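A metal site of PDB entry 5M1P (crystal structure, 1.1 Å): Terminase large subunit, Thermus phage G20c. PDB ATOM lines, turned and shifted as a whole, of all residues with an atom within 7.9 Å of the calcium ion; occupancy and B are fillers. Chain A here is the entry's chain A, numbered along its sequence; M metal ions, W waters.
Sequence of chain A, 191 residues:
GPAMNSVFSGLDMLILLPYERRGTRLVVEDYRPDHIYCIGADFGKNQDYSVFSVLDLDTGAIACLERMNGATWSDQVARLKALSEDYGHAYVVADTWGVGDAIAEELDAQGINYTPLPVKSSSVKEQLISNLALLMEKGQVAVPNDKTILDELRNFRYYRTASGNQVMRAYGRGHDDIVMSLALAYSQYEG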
ATOM      1  N   ALA A  41      12.858 -18.560   5.673  1.00  0.00           N
ATOM      2  CA  ALA A  41      14.164 -18.134   6.152  1.00  0.00           C
ATOM      3  C   ALA A  41      14.634 -16.885   5.426  1.00  0.00           C
ATOM      4  O   ALA A  41      14.847 -16.900   4.212  1.00  0.00           O
ATOM      5  CB  ALA A  41      15.160 -19.261   5.995  1.00  0.00           C
ATOM      6  N   ASP A  42      14.728 -15.818   6.226  1.00  0.00           N
ATOM      7  CA  ASP A  42      15.289 -14.528   5.873  1.00  0.00           C
ATOM      8  C   ASP A  42      16.615 -14.487   6.620  1.00  0.00           C
ATOM      9  O   ASP A  42      16.640 -14.476   7.850  1.00  0.00           O
ATOM     10  CB  ASP A  42      14.335 -13.409   6.347  1.00  0.00           C
ATOM     11  CG  ASP A  42      14.839 -12.015   6.024  1.00  0.00           C
ATOM     12  OD1 ASP A  42      15.682 -11.504   6.787  1.00  0.00           O
ATOM     13  OD2 ASP A  42      14.385 -11.424   5.046  1.00  0.00           O
ATOM     14  N   PHE A  43      17.718 -14.504   5.890  1.00  0.00           N
ATOM     15  CA  PHE A  43      19.044 -14.580   6.512  1.00  0.00           C
ATOM     16  C   PHE A  43      19.484 -13.248   7.088  1.00  0.00           C
ATOM     17  O   PHE A  43      18.929 -12.204   6.749  1.00  0.00           O
ATOM     18  CB  PHE A  43      20.067 -15.131   5.519  1.00  0.00           C
ATOM     19  CG  PHE A  43      19.851 -16.575   5.229  1.00  0.00           C
ATOM     20  CD1 PHE A  43      20.327 -17.536   6.098  1.00  0.00           C
ATOM     21  CD2 PHE A  43      19.088 -16.971   4.141  1.00  0.00           C
ATOM     22  CE1 PHE A  43      20.102 -18.888   5.855  1.00  0.00           C
ATOM     23  CE2 PHE A  43      18.857 -18.310   3.888  1.00  0.00           C
ATOM     24  CZ  PHE A  43      19.368 -19.257   4.753  1.00  0.00           C
ATOM     25  N   GLY A  44      20.433 -13.329   8.013  1.00  0.00           N
ATOM     26  CA  GLY A  44      21.127 -12.183   8.566  1.00  0.00           C
ATOM     27  C   GLY A  44      22.312 -11.952   7.659  1.00  0.00           C
ATOM     28  O   GLY A  44      23.393 -12.510   7.872  1.00  0.00           O
ATOM     29  N   LYS A  45      22.085 -11.185   6.603  1.00  0.00           N
ATOM     30  CA  LYS A  45      23.096 -10.972   5.569  1.00  0.00           C
ATOM     31  C   LYS A  45      24.320 -10.252   6.113  1.00  0.00           C
ATOM     32  O   LYS A  45      25.440 -10.675   5.889  1.00  0.00           O
ATOM     33  CB  LYS A  45      22.503 -10.212   4.370  1.00  0.00           C
ATOM     34  N   ASN A  46      24.099  -9.166   6.854  1.00  0.00           N
ATOM     35  CA  ASN A  46      25.165  -8.468   7.568  1.00  0.00           C
ATOM     36  C   ASN A  46      24.746  -8.202   9.030  1.00  0.00           C
ATOM     37  O   ASN A  46      24.714  -9.141   9.814  1.00  0.00           O
ATOM     38  CB  ASN A  46      25.597  -7.212   6.793  1.00  0.00           C
ATOM     39  CG  ASN A  46      26.775  -6.499   7.453  1.00  0.00           C
ATOM     40  OD1 ASN A  46      27.781  -7.136   7.775  1.00  0.00           O
ATOM     41  ND2 ASN A  46      26.646  -5.201   7.679  1.00  0.00           N
ATOM     42  N   GLN A  47      24.399  -6.958   9.399  1.00  0.00           N
ATOM     43  CA  GLN A  47      24.005  -6.637  10.782  1.00  0.00           C
ATOM     44  C   GLN A  47      22.495  -6.778  10.970  1.00  0.00           C
ATOM     45  O   GLN A  47      21.982  -6.655  12.101  1.00  0.00           O
ATOM     46  CB  GLN A  47      24.423  -5.217  11.158  1.00  0.00           C
ATOM     47  N   ASP A  48      21.772  -6.996   9.877  1.00  0.00           N
ATOM     48  CA  ASP A  48      20.334  -7.255   9.919  1.00  0.00           C
ATOM     49  C   ASP A  48      20.020  -8.577  10.621  1.00  0.00           C
ATOM     50  O   ASP A  48      20.865  -9.452  10.769  1.00  0.00           O
ATOM     51  CB  ASP A  48      19.733  -7.250   8.506  1.00  0.00           C
ATOM     52  CG  ASP A  48      20.366  -8.266   7.579  1.00  0.00           C
ATOM     53  OD1 ASP A  48      21.523  -8.053   7.188  1.00  0.00           O
ATOM     54  OD2 ASP A  48      19.703  -9.267   7.253  1.00  0.00           O
ATOM     55  N   TYR A  49      18.758  -8.711  11.021  1.00  0.00           N
ATOM     56  CA  TYR A  49      18.308  -9.926  11.676  1.00  0.00           C
ATOM     57  C   TYR A  49      18.146 -11.081  10.697  1.00  0.00           C
ATOM     58  O   TYR A  49      17.829 -10.902   9.509  1.00  0.00           O
ATOM     59  CB  TYR A  49      16.962  -9.689  12.403  1.00  0.00           C
ATOM     60  CG  TYR A  49      17.047  -8.706  13.544  1.00  0.00           C
ATOM     61  CD1 TYR A  49      16.870  -7.351  13.336  1.00  0.00           C
ATOM     62  CD2 TYR A  49      17.312  -9.134  14.846  1.00  0.00           C
ATOM     63  CE1 TYR A  49      16.971  -6.438  14.370  1.00  0.00           C
ATOM     64  CE2 TYR A  49      17.414  -8.227  15.893  1.00  0.00           C
ATOM     65  CZ  TYR A  49      17.252  -6.883  15.649  1.00  0.00           C
ATOM     66  OH  TYR A  49      17.330  -5.972  16.676  1.00  0.00           O
ATOM     67  N   SER A  50      18.371 -12.272  11.232  1.00  0.00           N
ATOM     68  CA  SER A  50      17.939 -13.511  10.610  1.00  0.00           C
ATOM     69  C   SER A  50      16.678 -13.941  11.308  1.00  0.00           C
ATOM     70  O   SER A  50      16.609 -13.861  12.526  1.00  0.00           O
ATOM     71  CB  SER A  50      19.000 -14.595  10.781  1.00  0.00           C
ATOM     72  OG  SER A  50      19.384 -14.773  12.135  1.00  0.00           O
ATOM     73  N   VAL A  51      15.678 -14.375  10.532  1.00  0.00           N
ATOM     74  CA  VAL A  51      14.419 -14.853  11.079  1.00  0.00           C
ATOM     75  C   VAL A  51      14.006 -16.131  10.371  1.00  0.00           C
ATOM     76  O   VAL A  51      13.860 -16.164   9.138  1.00  0.00           O
ATOM     77  CB  VAL A  51      13.309 -13.813  10.954  1.00  0.00           C
ATOM     78  CG1 VAL A  51      12.041 -14.309  11.640  1.00  0.00           C
ATOM     79  CG2 VAL A  51      13.756 -12.494  11.539  1.00  0.00           C
ATOM     80  N   MET A  68      17.575 -13.662  15.438  1.00  0.00           N
ATOM     81  CA  MET A  68      18.723 -13.044  16.083  1.00  0.00           C
ATOM     82  C   MET A  68      19.425 -12.149  15.089  1.00  0.00           C
ATOM     83  O   MET A  68      19.076 -12.116  13.934  1.00  0.00           O
ATOM     84  CB  MET A  68      19.675 -14.095  16.673  1.00  0.00           C
ATOM     85  CG  MET A  68      20.302 -15.031  15.649  1.00  0.00           C
ATOM     86  SD  MET A  68      19.165 -16.137  14.816  1.00  0.00           S
ATOM     87  CE  MET A  68      20.358 -17.102  13.871  1.00  0.00           C
ATOM     88  N   GLN A  76      23.955 -19.410  11.432  1.00  0.00           N
ATOM     89  CA  GLN A  76      22.599 -19.305  10.870  1.00  0.00           C
ATOM     90  C   GLN A  76      22.158 -20.588  10.185  1.00  0.00           C
ATOM     91  O   GLN A  76      21.047 -21.066  10.394  1.00  0.00           O
ATOM     92  CB  GLN A  76      22.500 -18.132   9.915  1.00  0.00           C
ATOM     93  CG  GLN A  76      22.635 -16.787  10.606  1.00  0.00           C
ATOM     94  CD  GLN A  76      22.552 -15.659   9.630  1.00  0.00           C
ATOM     95  OE1 GLN A  76      21.664 -15.641   8.768  1.00  0.00           O
ATOM     96  NE2 GLN A  76      23.479 -14.714   9.726  1.00  0.00           N
ATOM     97  N   ASP A  95      15.188 -17.333   1.197  1.00  0.00           N
ATOM     98  CA  ASP A  95      15.483 -16.186   0.354  1.00  0.00           C
ATOM     99  C   ASP A  95      16.975 -16.141   0.142  1.00  0.00           C
ATOM    100  O   ASP A  95      17.727 -15.611   0.949  1.00  0.00           O
ATOM    101  CB  ASP A  95      14.987 -14.872   0.937  1.00  0.00           C
ATOM    102  CG  ASP A  95      15.427 -13.665   0.111  1.00  0.00           C
ATOM    103  OD1 ASP A  95      15.887 -13.828  -1.049  1.00  0.00           O
ATOM    104  OD2 ASP A  95      15.320 -12.536   0.625  1.00  0.00           O
ATOM    105  N   HIS A 175      12.717  -2.349  10.247  1.00  0.00           N
ATOM    106  CA  HIS A 175      13.170  -3.628   9.719  1.00  0.00           C
ATOM    107  C   HIS A 175      11.985  -4.386   9.148  1.00  0.00           C
ATOM    108  O   HIS A 175      10.833  -4.137   9.525  1.00  0.00           O
ATOM    109  CB  HIS A 175      13.799  -4.479  10.825  1.00  0.00           C
ATOM    110  CG  HIS A 175      14.715  -3.734  11.743  1.00  0.00           C
ATOM    111  ND1 HIS A 175      15.795  -3.009  11.293  1.00  0.00           N
ATOM    112  CD2 HIS A 175      14.705  -3.602  13.087  1.00  0.00           C
ATOM    113  CE1 HIS A 175      16.416  -2.465  12.321  1.00  0.00           C
ATOM    114  NE2 HIS A 175      15.773  -2.810  13.425  1.00  0.00           N
ATOM    115  N   ASP A 176      12.270  -5.373   8.292  1.00  0.00           N
ATOM    116  CA  ASP A 176      11.213  -6.220   7.746  1.00  0.00           C
ATOM    117  C   ASP A 176      11.561  -7.712   7.718  1.00  0.00           C
ATOM    118  O   ASP A 176      10.896  -8.469   7.026  1.00  0.00           O
ATOM    119  CB  ASP A 176      10.792  -5.742   6.343  1.00  0.00           C
ATOM    120  CG  ASP A 176      11.883  -5.920   5.309  1.00  0.00           C
ATOM    121  OD1 ASP A 176      12.959  -6.442   5.637  1.00  0.00           O
ATOM    122  OD2 ASP A 176      11.637  -5.525   4.138  1.00  0.00           O
ATOM    123  N   ASP A 177      12.566  -8.125   8.502  1.00  0.00           N
ATOM    124  CA  ASP A 177      13.050  -9.508   8.427  1.00  0.00           C
ATOM    125  C   ASP A 177      11.977 -10.488   8.893  1.00  0.00           C
ATOM    126  O   ASP A 177      11.875 -11.597   8.376  1.00  0.00           O
ATOM    127  CB  ASP A 177      14.296  -9.725   9.287  1.00  0.00           C
ATOM    128  CG  ASP A 177      15.281  -8.592   9.181  1.00  0.00           C
ATOM    129  OD1 ASP A 177      15.180  -7.652  10.000  1.00  0.00           O
ATOM    130  OD2 ASP A 177      16.144  -8.632   8.287  1.00  0.00           O
ATOM    131  N   ILE A 178      11.197 -10.082   9.904  1.00  0.00           N
ATOM    132  CA  ILE A 178      10.120 -10.936  10.408  1.00  0.00           C
ATOM    133  C   ILE A 178       9.007 -11.028   9.366  1.00  0.00           C
ATOM    134  O   ILE A 178       8.501 -12.105   9.053  1.00  0.00           O
ATOM    135  CB  ILE A 178       9.526 -10.417  11.731  1.00  0.00           C
ATOM    136  CG1 ILE A 178      10.590 -10.375  12.831  1.00  0.00           C
ATOM    137  CG2 ILE A 178       8.323 -11.275  12.156  1.00  0.00           C
ATOM    138  CD1 ILE A 178      10.159  -9.604  14.067  1.00  0.00           C
ATOM    139  N   MET A 180       9.181 -10.663   6.133  1.00  0.00           N
ATOM    140  CA  MET A 180       9.617 -11.450   4.998  1.00  0.00           C
ATOM    141  C   MET A 180       9.709 -12.939   5.332  1.00  0.00           C
ATOM    142  O   MET A 180       9.296 -13.769   4.511  1.00  0.00           O
ATOM    143  CB  MET A 180      10.939 -10.909   4.443  1.00  0.00           C
ATOM    144  CG  MET A 180      10.811  -9.534   3.780  1.00  0.00           C
ATOM    145  SD  MET A 180       9.427  -9.355   2.637  1.00  0.00           S
ATOM    146  CE  MET A 180       9.689 -10.707   1.499  1.00  0.00           C
HETATM  147 CA    CA M   1      17.571 -10.312   7.315  1.00  0.00          CA
HETATM  148  O   HOH W   1      17.293  -9.087   5.348  1.00  0.00           O
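The calcium ion is bound by O of Tyr 49 (2.3 Å), OD1 of Asp 42 (2.3 Å), water W1 (2.3 Å), OD2 of Asp 48 (2.4 Å), O of Phe 43 (2.4 Å) and OD2 of Asp 177 (2.4 Å).
The backbone carbonyl oxygen (O) of Asp 42 is in hydrogen-bond range of the backbone NH (N) of Val 51 (2.9 Å).
The side-chain carboxylate of Asp 48 lies within hydrogen-bond range of the backbone NH of Lys 45 (3.2 Å).
N of Asn 46 lies within hydrogen-bond range of OD1 of Asp 48 (2.8 Å).
Five residues have an atom within 4 Å of the calcium ion: Asp 42, Phe 43, Asp 48, Tyr 49 and Asp 177.
The nearest printed residue that does not touch the calcium ion is Gly 44 (4.2 Å).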
